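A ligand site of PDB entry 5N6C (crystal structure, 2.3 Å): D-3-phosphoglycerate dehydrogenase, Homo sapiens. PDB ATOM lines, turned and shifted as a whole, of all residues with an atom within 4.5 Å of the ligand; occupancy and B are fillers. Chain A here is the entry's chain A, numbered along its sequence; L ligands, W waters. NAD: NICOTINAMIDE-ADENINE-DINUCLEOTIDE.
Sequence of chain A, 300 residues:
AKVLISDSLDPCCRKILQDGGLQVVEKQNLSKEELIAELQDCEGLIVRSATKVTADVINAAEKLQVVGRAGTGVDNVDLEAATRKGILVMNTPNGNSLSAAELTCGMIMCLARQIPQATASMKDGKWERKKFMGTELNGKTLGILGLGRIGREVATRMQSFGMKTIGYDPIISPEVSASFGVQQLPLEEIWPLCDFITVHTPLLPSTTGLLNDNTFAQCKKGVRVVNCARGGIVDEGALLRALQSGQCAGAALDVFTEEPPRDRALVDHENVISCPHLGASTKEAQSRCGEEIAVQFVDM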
ATOM      1  N   THR A  72      -0.864   8.129 -20.756  1.00  0.00           N
ATOM      2  CA  THR A  72       0.406   8.787 -20.435  1.00  0.00           C
ATOM      3  C   THR A  72       1.340   8.791 -21.600  1.00  0.00           C
ATOM      4  O   THR A  72       1.160   8.019 -22.559  1.00  0.00           O
ATOM      5  CB  THR A  72       1.166   8.101 -19.332  1.00  0.00           C
ATOM      6  OG1 THR A  72       1.443   6.726 -19.698  1.00  0.00           O
ATOM      7  CG2 THR A  72       0.329   8.283 -18.001  1.00  0.00           C
ATOM      8  N   PRO A  93      -1.858  12.366 -17.188  1.00  0.00           N
ATOM      9  CA  PRO A  93      -0.845  11.699 -16.374  1.00  0.00           C
ATOM     10  C   PRO A  93      -1.319  11.090 -15.054  1.00  0.00           C
ATOM     11  O   PRO A  93      -0.555  10.313 -14.449  1.00  0.00           O
ATOM     12  CB  PRO A  93       0.158  12.850 -16.098  1.00  0.00           C
ATOM     13  CG  PRO A  93      -0.715  14.085 -16.056  1.00  0.00           C
ATOM     14  CD  PRO A  93      -1.648  13.832 -17.228  1.00  0.00           C
ATOM     15  N   ASN A  96      -4.657   6.893 -14.931  1.00  0.00           N
ATOM     16  CA  ASN A  96      -4.288   5.503 -15.043  1.00  0.00           C
ATOM     17  C   ASN A  96      -3.463   4.863 -13.986  1.00  0.00           C
ATOM     18  O   ASN A  96      -3.199   3.643 -14.059  1.00  0.00           O
ATOM     19  CB  ASN A  96      -3.342   5.374 -16.234  1.00  0.00           C
ATOM     20  CG  ASN A  96      -4.083   5.322 -17.507  1.00  0.00           C
ATOM     21  OD1 ASN A  96      -5.240   4.943 -17.486  1.00  0.00           O
ATOM     22  ND2 ASN A  96      -3.440   5.710 -18.621  1.00  0.00           N
ATOM     23  N   ALA A 100      -2.471   0.651 -13.347  1.00  0.00           N
ATOM     24  CA  ALA A 100      -1.104   0.185 -13.660  1.00  0.00           C
ATOM     25  C   ALA A 100      -0.404  -0.378 -12.451  1.00  0.00           C
ATOM     26  O   ALA A 100       0.249  -1.439 -12.567  1.00  0.00           O
ATOM     27  CB  ALA A 100      -0.315   1.306 -14.237  1.00  0.00           C
ATOM     28  N   LEU A 145      12.278   0.868  -9.384  1.00  0.00           N
ATOM     29  CA  LEU A 145      13.067   1.900 -10.020  1.00  0.00           C
ATOM     30  C   LEU A 145      12.096   2.877 -10.575  1.00  0.00           C
ATOM     31  O   LEU A 145      11.298   2.497 -11.493  1.00  0.00           O
ATOM     32  CB  LEU A 145      13.946   1.249 -11.113  1.00  0.00           C
ATOM     33  CG  LEU A 145      14.754   0.000 -10.707  1.00  0.00           C
ATOM     34  CD1 LEU A 145      15.697  -0.377 -11.757  1.00  0.00           C
ATOM     35  CD2 LEU A 145      15.599   0.195  -9.348  1.00  0.00           C
ATOM     36  N   GLY A 146      12.085   4.093 -10.047  1.00  0.00           N
ATOM     37  CA  GLY A 146      11.007   5.022 -10.376  1.00  0.00           C
ATOM     38  C   GLY A 146      10.006   5.085  -9.218  1.00  0.00           C
ATOM     39  O   GLY A 146       9.245   4.123  -8.990  1.00  0.00           O
ATOM     40  N   LEU A 147      10.015   6.184  -8.504  1.00  0.00           N
ATOM     41  CA  LEU A 147       9.183   6.297  -7.334  1.00  0.00           C
ATOM     42  C   LEU A 147       8.276   7.469  -7.437  1.00  0.00           C
ATOM     43  O   LEU A 147       8.108   8.153  -6.400  1.00  0.00           O
ATOM     44  CB  LEU A 147      10.069   6.393  -6.014  1.00  0.00           C
ATOM     45  CG  LEU A 147      11.105   5.251  -5.839  1.00  0.00           C
ATOM     46  CD1 LEU A 147      12.219   5.476  -4.815  1.00  0.00           C
ATOM     47  CD2 LEU A 147      10.355   3.907  -5.576  1.00  0.00           C
ATOM     48  N   GLY A 148       7.655   7.652  -8.596  1.00  0.00           N
ATOM     49  CA  GLY A 148       6.613   8.649  -8.818  1.00  0.00           C
ATOM     50  C   GLY A 148       5.216   8.079  -8.496  1.00  0.00           C
ATOM     51  O   GLY A 148       5.060   7.341  -7.599  1.00  0.00           O
ATOM     52  N   ARG A 149       4.216   8.434  -9.267  1.00  0.00           N
ATOM     53  CA  ARG A 149       2.805   7.994  -9.137  1.00  0.00           C
ATOM     54  C   ARG A 149       2.618   6.512  -8.986  1.00  0.00           C
ATOM     55  O   ARG A 149       2.014   6.051  -8.022  1.00  0.00           O
ATOM     56  CB  ARG A 149       1.963   8.460 -10.318  1.00  0.00           C
ATOM     57  CG  ARG A 149       1.755   9.976 -10.392  1.00  0.00           C
ATOM     58  CD  ARG A 149       1.093  10.303 -11.714  1.00  0.00           C
ATOM     59  NE  ARG A 149       0.840  11.704 -11.944  1.00  0.00           N
ATOM     60  CZ  ARG A 149       1.778  12.553 -12.426  1.00  0.00           C
ATOM     61  NH1 ARG A 149       3.083  12.153 -12.633  1.00  0.00           N
ATOM     62  NH2 ARG A 149       1.470  13.853 -12.629  1.00  0.00           N
ATOM     63  N   ILE A 150       3.268   5.728  -9.803  1.00  0.00           N
ATOM     64  CA  ILE A 150       2.985   4.311  -9.796  1.00  0.00           C
ATOM     65  C   ILE A 150       3.879   3.556  -8.887  1.00  0.00           C
ATOM     66  O   ILE A 150       3.435   2.656  -8.196  1.00  0.00           O
ATOM     67  CB  ILE A 150       3.041   3.729 -11.250  1.00  0.00           C
ATOM     68  CG1 ILE A 150       1.866   4.279 -12.087  1.00  0.00           C
ATOM     69  CG2 ILE A 150       2.927   2.174 -11.275  1.00  0.00           C
ATOM     70  CD1 ILE A 150       2.145   4.183 -13.566  1.00  0.00           C
ATOM     71  N   GLY A 151       5.177   3.900  -8.920  1.00  0.00           N
ATOM     72  CA  GLY A 151       6.170   3.275  -8.068  1.00  0.00           C
ATOM     73  C   GLY A 151       5.784   3.265  -6.572  1.00  0.00           C
ATOM     74  O   GLY A 151       5.906   2.233  -5.963  1.00  0.00           O
ATOM     75  N   TYR A 168      15.175   3.433  -6.229  1.00  0.00           N
ATOM     76  CA  TYR A 168      16.008   4.514  -6.694  1.00  0.00           C
ATOM     77  C   TYR A 168      15.189   5.458  -7.557  1.00  0.00           C
ATOM     78  O   TYR A 168      14.397   5.026  -8.331  1.00  0.00           O
ATOM     79  CB  TYR A 168      17.152   3.958  -7.580  1.00  0.00           C
ATOM     80  CG  TYR A 168      17.953   5.076  -8.138  1.00  0.00           C
ATOM     81  CD1 TYR A 168      18.785   5.876  -7.300  1.00  0.00           C
ATOM     82  CD2 TYR A 168      17.876   5.385  -9.453  1.00  0.00           C
ATOM     83  CE1 TYR A 168      19.513   6.945  -7.807  1.00  0.00           C
ATOM     84  CE2 TYR A 168      18.588   6.465  -9.981  1.00  0.00           C
ATOM     85  CZ  TYR A 168      19.397   7.240  -9.157  1.00  0.00           C
ATOM     86  OH  TYR A 168      20.084   8.260  -9.767  1.00  0.00           O
ATOM     87  N   ASP A 169      15.376   6.761  -7.365  1.00  0.00           N
ATOM     88  CA  ASP A 169      14.707   7.792  -8.141  1.00  0.00           C
ATOM     89  C   ASP A 169      15.592   9.064  -8.009  1.00  0.00           C
ATOM     90  O   ASP A 169      15.924   9.520  -6.895  1.00  0.00           O
ATOM     91  CB  ASP A 169      13.304   8.052  -7.608  1.00  0.00           C
ATOM     92  CG  ASP A 169      12.499   8.954  -8.495  1.00  0.00           C
ATOM     93  OD1 ASP A 169      12.986  10.048  -8.747  1.00  0.00           O
ATOM     94  OD2 ASP A 169      11.382   8.594  -8.960  1.00  0.00           O
ATOM     95  N   PRO A 170      15.987   9.655  -9.138  1.00  0.00           N
ATOM     96  CA  PRO A 170      16.936  10.777  -9.081  1.00  0.00           C
ATOM     97  C   PRO A 170      16.319  12.065  -8.582  1.00  0.00           C
ATOM     98  O   PRO A 170      16.986  13.011  -8.349  1.00  0.00           O
ATOM     99  CB  PRO A 170      17.370  10.910 -10.517  1.00  0.00           C
ATOM    100  CG  PRO A 170      16.182  10.265 -11.340  1.00  0.00           C
ATOM    101  CD  PRO A 170      15.740   9.156 -10.492  1.00  0.00           C
ATOM    102  N   ILE A 171      15.007  12.111  -8.458  1.00  0.00           N
ATOM    103  CA  ILE A 171      14.325  13.359  -8.076  1.00  0.00           C
ATOM    104  C   ILE A 171      13.707  13.320  -6.620  1.00  0.00           C
ATOM    105  O   ILE A 171      13.388  14.323  -6.073  1.00  0.00           O
ATOM    106  CB  ILE A 171      13.176  13.600  -9.098  1.00  0.00           C
ATOM    107  CG1 ILE A 171      13.705  13.606 -10.561  1.00  0.00           C
ATOM    108  CG2 ILE A 171      12.495  14.928  -8.851  1.00  0.00           C
ATOM    109  CD1 ILE A 171      14.740  14.617 -10.892  1.00  0.00           C
ATOM    110  N   ILE A 172      13.465  12.119  -6.100  1.00  0.00           N
ATOM    111  CA  ILE A 172      12.755  11.945  -4.852  1.00  0.00           C
ATOM    112  C   ILE A 172      13.863  11.815  -3.785  1.00  0.00           C
ATOM    113  O   ILE A 172      14.780  10.963  -3.956  1.00  0.00           O
ATOM    114  CB  ILE A 172      11.875  10.723  -4.901  1.00  0.00           C
ATOM    115  CG1 ILE A 172      10.838  10.760  -6.056  1.00  0.00           C
ATOM    116  CG2 ILE A 172      11.162  10.565  -3.543  1.00  0.00           C
ATOM    117  CD1 ILE A 172       9.852  11.923  -5.984  1.00  0.00           C
ATOM    118  N   HIS A 200       9.326   1.607 -13.268  1.00  0.00           N
ATOM    119  CA  HIS A 200       8.267   2.561 -13.293  1.00  0.00           C
ATOM    120  C   HIS A 200       8.752   3.926 -13.599  1.00  0.00           C
ATOM    121  O   HIS A 200       8.382   4.916 -12.980  1.00  0.00           O
ATOM    122  CB  HIS A 200       7.420   2.561 -12.017  1.00  0.00           C
ATOM    123  CG  HIS A 200       6.856   1.230 -11.678  1.00  0.00           C
ATOM    124  ND1 HIS A 200       5.731   0.723 -12.257  1.00  0.00           N
ATOM    125  CD2 HIS A 200       7.249   0.298 -10.785  1.00  0.00           C
ATOM    126  CE1 HIS A 200       5.508  -0.493 -11.821  1.00  0.00           C
ATOM    127  NE2 HIS A 200       6.422  -0.807 -10.958  1.00  0.00           N
ATOM    128  N   THR A 201       9.587   3.962 -14.619  1.00  0.00           N
ATOM    129  CA  THR A 201      10.214   5.212 -15.093  1.00  0.00           C
ATOM    130  C   THR A 201       9.622   5.568 -16.445  1.00  0.00           C
ATOM    131  O   THR A 201       9.008   4.714 -17.092  1.00  0.00           O
ATOM    132  CB  THR A 201      11.736   5.066 -15.282  1.00  0.00           C
ATOM    133  OG1 THR A 201      11.989   4.175 -16.395  1.00  0.00           O
ATOM    134  CG2 THR A 201      12.408   4.540 -13.971  1.00  0.00           C
ATOM    135  N   PRO A 202       9.773   6.835 -16.845  1.00  0.00           N
ATOM    136  CA  PRO A 202       9.545   7.111 -18.255  1.00  0.00           C
ATOM    137  C   PRO A 202      10.661   6.521 -19.128  1.00  0.00           C
ATOM    138  O   PRO A 202      11.615   5.993 -18.595  1.00  0.00           O
ATOM    139  CB  PRO A 202       9.455   8.597 -18.312  1.00  0.00           C
ATOM    140  CG  PRO A 202      10.282   9.030 -17.161  1.00  0.00           C
ATOM    141  CD  PRO A 202      10.207   8.022 -16.095  1.00  0.00           C
ATOM    142  N   LEU A 203      10.436   6.442 -20.453  1.00  0.00           N
ATOM    143  CA  LEU A 203      11.465   5.993 -21.445  1.00  0.00           C
ATOM    144  C   LEU A 203      12.235   7.188 -21.983  1.00  0.00           C
ATOM    145  O   LEU A 203      11.692   8.084 -22.590  1.00  0.00           O
ATOM    146  CB  LEU A 203      10.902   5.133 -22.619  1.00  0.00           C
ATOM    147  CG  LEU A 203      11.945   4.642 -23.635  1.00  0.00           C
ATOM    148  CD1 LEU A 203      12.802   3.511 -23.065  1.00  0.00           C
ATOM    149  CD2 LEU A 203      11.310   4.257 -24.991  1.00  0.00           C
ATOM    150  N   THR A 207      17.147   5.854 -19.520  1.00  0.00           N
ATOM    151  CA  THR A 207      16.387   4.655 -19.030  1.00  0.00           C
ATOM    152  C   THR A 207      16.273   3.533 -20.047  1.00  0.00           C
ATOM    153  O   THR A 207      15.794   2.467 -19.718  1.00  0.00           O
ATOM    154  CB  THR A 207      15.013   5.021 -18.480  1.00  0.00           C
ATOM    155  OG1 THR A 207      14.243   5.642 -19.474  1.00  0.00           O
ATOM    156  CG2 THR A 207      15.201   6.057 -17.245  1.00  0.00           C
ATOM    157  N   LEU A 210      18.073   0.222 -18.920  1.00  0.00           N
ATOM    158  CA  LEU A 210      18.439   0.423 -17.541  1.00  0.00           C
ATOM    159  C   LEU A 210      18.754  -0.943 -16.866  1.00  0.00           C
ATOM    160  O   LEU A 210      19.665  -1.053 -16.125  1.00  0.00           O
ATOM    161  CB  LEU A 210      17.273   1.093 -16.849  1.00  0.00           C
ATOM    162  CG  LEU A 210      17.440   1.627 -15.462  1.00  0.00           C
ATOM    163  CD1 LEU A 210      18.459   2.709 -15.374  1.00  0.00           C
ATOM    164  CD2 LEU A 210      16.080   2.135 -14.983  1.00  0.00           C
ATOM    165  N   CYS A 228       5.871  -3.191 -16.533  1.00  0.00           N
ATOM    166  CA  CYS A 228       4.615  -2.568 -16.764  1.00  0.00           C
ATOM    167  C   CYS A 228       4.777  -1.074 -17.036  1.00  0.00           C
ATOM    168  O   CYS A 228       3.796  -0.354 -16.938  1.00  0.00           O
ATOM    169  CB  CYS A 228       3.620  -2.798 -15.625  1.00  0.00           C
ATOM    170  SG  CYS A 228       3.106  -4.560 -15.596  1.00  0.00           S
ATOM    171  N   ALA A 229       5.940  -0.652 -17.501  1.00  0.00           N
ATOM    172  CA  ALA A 229       6.139   0.758 -17.850  1.00  0.00           C
ATOM    173  C   ALA A 229       6.187   1.038 -19.369  1.00  0.00           C
ATOM    174  O   ALA A 229       5.172   1.419 -19.937  1.00  0.00           O
ATOM    175  CB  ALA A 229       7.410   1.313 -17.133  1.00  0.00           C
ATOM    176  N   ARG A 230       7.347   0.914 -19.998  1.00  0.00           N
ATOM    177  CA  ARG A 230       7.482   1.089 -21.458  1.00  0.00           C
ATOM    178  C   ARG A 230       8.515   0.094 -21.947  1.00  0.00           C
ATOM    179  O   ARG A 230       9.510  -0.233 -21.207  1.00  0.00           O
ATOM    180  CB  ARG A 230       7.978   2.462 -21.887  1.00  0.00           C
ATOM    181  CG  ARG A 230       6.994   3.606 -21.866  1.00  0.00           C
ATOM    182  CD  ARG A 230       5.943   3.361 -22.920  1.00  0.00           C
ATOM    183  NE  ARG A 230       4.805   4.313 -22.853  1.00  0.00           N
ATOM    184  CZ  ARG A 230       3.670   4.165 -22.111  1.00  0.00           C
ATOM    185  NH1 ARG A 230       3.406   3.081 -21.361  1.00  0.00           N
ATOM    186  NH2 ARG A 230       2.741   5.118 -22.250  1.00  0.00           N
ATOM    187  N   ASP A 254       4.133  -6.276 -19.995  1.00  0.00           N
ATOM    188  CA  ASP A 254       2.897  -5.634 -20.369  1.00  0.00           C
ATOM    189  C   ASP A 254       3.228  -4.756 -21.543  1.00  0.00           C
ATOM    190  O   ASP A 254       2.318  -4.343 -22.226  1.00  0.00           O
ATOM    191  CB  ASP A 254       2.264  -4.746 -19.241  1.00  0.00           C
ATOM    192  CG  ASP A 254       0.897  -4.222 -19.605  1.00  0.00           C
ATOM    193  OD1 ASP A 254       0.017  -5.065 -19.946  1.00  0.00           O
ATOM    194  OD2 ASP A 254       0.584  -2.980 -19.601  1.00  0.00           O
ATOM    195  N   VAL A 255       4.494  -4.483 -21.848  1.00  0.00           N
ATOM    196  CA  VAL A 255       4.900  -3.510 -22.871  1.00  0.00           C
ATOM    197  C   VAL A 255       6.156  -4.000 -23.623  1.00  0.00           C
ATOM    198  O   VAL A 255       6.958  -4.814 -23.147  1.00  0.00           O
ATOM    199  CB  VAL A 255       5.237  -2.148 -22.213  1.00  0.00           C
ATOM    200  CG1 VAL A 255       3.986  -1.504 -21.705  1.00  0.00           C
ATOM    201  CG2 VAL A 255       6.319  -2.293 -21.095  1.00  0.00           C
ATOM    202  N   HIS A 277      -0.394  -4.896 -23.322  1.00  0.00           N
ATOM    203  CA  HIS A 277      -0.457  -3.522 -22.841  1.00  0.00           C
ATOM    204  C   HIS A 277      -1.832  -3.218 -22.187  1.00  0.00           C
ATOM    205  O   HIS A 277      -2.560  -2.343 -22.580  1.00  0.00           O
ATOM    206  CB  HIS A 277      -0.080  -2.573 -23.993  1.00  0.00           C
ATOM    207  CG  HIS A 277       0.274  -1.183 -23.560  1.00  0.00           C
ATOM    208  ND1 HIS A 277       1.142  -0.391 -24.244  1.00  0.00           N
ATOM    209  CD2 HIS A 277      -0.079  -0.468 -22.465  1.00  0.00           C
ATOM    210  CE1 HIS A 277       1.302   0.766 -23.628  1.00  0.00           C
ATOM    211  NE2 HIS A 277       0.523   0.762 -22.575  1.00  0.00           N
ATOM    212  N   GLY A 279      -2.235  -2.305 -18.852  1.00  0.00           N
ATOM    213  CA  GLY A 279      -2.025  -1.596 -17.549  1.00  0.00           C
ATOM    214  C   GLY A 279      -3.051  -0.516 -17.244  1.00  0.00           C
ATOM    215  O   GLY A 279      -3.447  -0.338 -16.079  1.00  0.00           O
ATOM    216  N   ALA A 280      -3.510   0.156 -18.299  1.00  0.00           N
ATOM    217  CA  ALA A 280      -4.585   1.165 -18.211  1.00  0.00           C
ATOM    218  C   ALA A 280      -5.981   0.637 -18.597  1.00  0.00           C
ATOM    219  O   ALA A 280      -6.973   1.374 -18.569  1.00  0.00           O
ATOM    220  CB  ALA A 280      -4.249   2.367 -19.072  1.00  0.00           C
HETATM  221  PA  NAD L   1       5.757   9.638 -12.999  1.00  0.00           P
HETATM  222  O1A NAD L   1       6.149  10.846 -13.782  1.00  0.00           O
HETATM  223  O2A NAD L   1       4.696   9.909 -11.973  1.00  0.00           O
HETATM  224  O5B NAD L   1       7.051   9.028 -12.398  1.00  0.00           O
HETATM  225  C5B NAD L   1       8.156   8.707 -13.171  1.00  0.00           C
HETATM  226  C4B NAD L   1       9.342   8.633 -12.205  1.00  0.00           C
HETATM  227  O4B NAD L   1      10.456   7.960 -12.758  1.00  0.00           O
HETATM  228  C3B NAD L   1       9.794  10.037 -11.762  1.00  0.00           C
HETATM  229  O3B NAD L   1       9.681  10.216 -10.340  1.00  0.00           O
HETATM  230  C2B NAD L   1      11.237  10.106 -12.193  1.00  0.00           C
HETATM  231  O2B NAD L   1      12.157  10.746 -11.288  1.00  0.00           O
HETATM  232  C1B NAD L   1      11.589   8.644 -12.214  1.00  0.00           C
HETATM  233  N9A NAD L   1      12.864   8.420 -12.901  1.00  0.00           N
HETATM  234  C8A NAD L   1      13.332   9.203 -13.903  1.00  0.00           C
HETATM  235  N7A NAD L   1      14.539   8.692 -14.292  1.00  0.00           N
HETATM  236  C5A NAD L   1      14.811   7.617 -13.558  1.00  0.00           C
HETATM  237  C6A NAD L   1      15.910   6.747 -13.489  1.00  0.00           C
HETATM  238  N6A NAD L   1      16.915   6.959 -14.349  1.00  0.00           N
HETATM  239  N1A NAD L   1      15.886   5.723 -12.600  1.00  0.00           N
HETATM  240  C2A NAD L   1      14.857   5.622 -11.749  1.00  0.00           C
HETATM  241  N3A NAD L   1      13.842   6.487 -11.760  1.00  0.00           N
HETATM  242  C4A NAD L   1      13.725   7.455 -12.636  1.00  0.00           C
HETATM  243  O3  NAD L   1       5.367   8.383 -13.951  1.00  0.00           O
HETATM  244  PN  NAD L   1       4.237   7.275 -13.658  1.00  0.00           P
HETATM  245  O1N NAD L   1       2.955   8.016 -13.772  1.00  0.00           O
HETATM  246  O2N NAD L   1       4.483   6.393 -12.502  1.00  0.00           O
HETATM  247  O5D NAD L   1       4.607   6.239 -14.836  1.00  0.00           O
HETATM  248  C5D NAD L   1       5.763   5.480 -14.868  1.00  0.00           C
HETATM  249  C4D NAD L   1       5.860   4.643 -16.152  1.00  0.00           C
HETATM  250  O4D NAD L   1       4.800   3.678 -16.358  1.00  0.00           O
HETATM  251  C3D NAD L   1       5.889   5.544 -17.389  1.00  0.00           C
HETATM  252  O3D NAD L   1       6.833   5.005 -18.334  1.00  0.00           O
HETATM  253  C2D NAD L   1       4.449   5.455 -17.850  1.00  0.00           C
HETATM  254  O2D NAD L   1       4.316   5.774 -19.214  1.00  0.00           O
HETATM  255  C1D NAD L   1       4.157   4.004 -17.607  1.00  0.00           C
HETATM  256  N1N NAD L   1       2.695   3.642 -17.680  1.00  0.00           N
HETATM  257  C2N NAD L   1       2.378   2.401 -18.138  1.00  0.00           C
HETATM  258  C3N NAD L   1       1.040   1.994 -18.237  1.00  0.00           C
HETATM  259  C7N NAD L   1       0.684   0.690 -18.827  1.00  0.00           C
HETATM  260  O7N NAD L   1       1.408  -0.313 -18.800  1.00  0.00           O
HETATM  261  N7N NAD L   1      -0.497   0.652 -19.397  1.00  0.00           N
HETATM  262  C4N NAD L   1       0.027   2.849 -17.830  1.00  0.00           C
HETATM  263  C5N NAD L   1       0.411   4.102 -17.290  1.00  0.00           C
HETATM  264  C6N NAD L   1       1.747   4.457 -17.229  1.00  0.00           C
HETATM  265  O   HOH W   1       6.593   5.780 -10.766  1.00  0.00           O
HETATM  266  O   HOH W   2      16.719   9.162 -15.687  1.00  0.00           O
HETATM  267  O   HOH W   3       4.410   1.522 -14.715  1.00  0.00           O
HETATM  268  O   HOH W   4       0.194   7.451 -14.244  1.00  0.00           O
HETATM  269  O   HOH W   5      19.706   5.543 -13.645  1.00  0.00           O
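The backbone carbonyl oxygen (O) of Thr 201 lies within hydrogen-bond range of an oxygen (O3D) of the ligand, at 2.5 Å.
An oxygen (O3B) of the ligand sits at hydrogen-bond distance from the side-chain carboxylate of Asp 169, at 2.7 Å.
An oxygen (O2A) of the ligand is in hydrogen-bond range of the backbone NH of Arg 149 (3.1 Å).
NH1 of Arg 149 lies within salt-bridge range of O2A of the ligand, at 2.8 Å.
The backbone NH of Ile 150 lies within hydrogen-bond range of an oxygen (O2N) of the ligand (3.0 Å).
The side-chain hydroxyl (OG1) of Thr 72 is in hydrogen-bond range of an oxygen (O2D) of the ligand, at 3.1 Å.
A nitrogen (N7N) of the ligand sits close to a ring nitrogen (NE2) of His 277 (3.3 Å).
O2D of the ligand lies close to NH2 of Arg 230, 3.5 Å away.
A nitrogen (N3A) of the ligand is in hydrogen-bond range of the backbone NH (N) of Gly 146 (3.4 Å).
OD1 of Asp 169 lies within hydrogen-bond range of N of Ile 171 (2.9 Å).
The side-chain carboxylate (OD2) of Asp 169 is in hydrogen-bond range of the backbone NH (N) of Leu 147 (2.8 Å).
OD1 of Asp 169 is in hydrogen-bond range of N of Ile 172, at 3.4 Å.
O of Pro 93 lies within hydrogen-bond range of NE of Arg 149 (3.2 Å).
The backbone NH of His 277 sits close to the backbone carbonyl oxygen of Asp 254.
The side-chain hydroxyl (OG1) of Thr 72 sits at hydrogen-bond distance from the guanidinium group (NH2) of Arg 230, 3.3 Å away.
The backbone carbonyl oxygen of Gly 279 sits at hydrogen-bond distance from the backbone NH of Ala 100 (3.1 Å).
N of Gly 146 is in hydrogen-bond range of O of Tyr 168 (3.0 Å).
The backbone carbonyl oxygen (O) of Cys 228 lies close to an oxygen (O7N) of the ligand, at 3.0 Å.
OD2 of Asp 254 lies close to O7N of the ligand (2.9 Å).
N of Gly 279 lies close to N7N of the ligand (3.5 Å).
A nitrogen (N7N) of the ligand lies close to the backbone NH (N) of Ala 280 (3.2 Å).
CB of Ala 100 touches C4N of the ligand (3.9 Å).
CA of Gly 148 touches O5B of the ligand (3.6 Å).
O of Tyr 168 touches C2A of the ligand, at 3.5 Å.
CD of Pro 170 touches C4A of the ligand (3.4 Å).
CG1 of Ile 171 touches O2B of the ligand, at 3.3 Å.
His 200 touches the ligand (O to C5D, 3.3 Å).
Pro 202 touches the ligand (CD to O4B, 3.3 Å).
CG2 of Thr 207 touches N6A of the ligand, at 3.5 Å.
Ala 229 touches the ligand.
Hydrophobic or aromatic side chains that line the ligand: Ala 100, Ile 150, Tyr 168, Pro 170, Ile 171, Pro 202, Ala 229 and His 277.
Water W3 lies within hydrogen-bond range of an oxygen (O4D) of the ligand (2.7 Å), a ring nitrogen (ND1) of His 200 (2.9 Å) and the backbone carbonyl oxygen of Cys 228 (3.0 Å).
Water W4 lies within hydrogen-bond range of O1N of the ligand (2.9 Å) and O of Pro 93 (3.0 Å).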
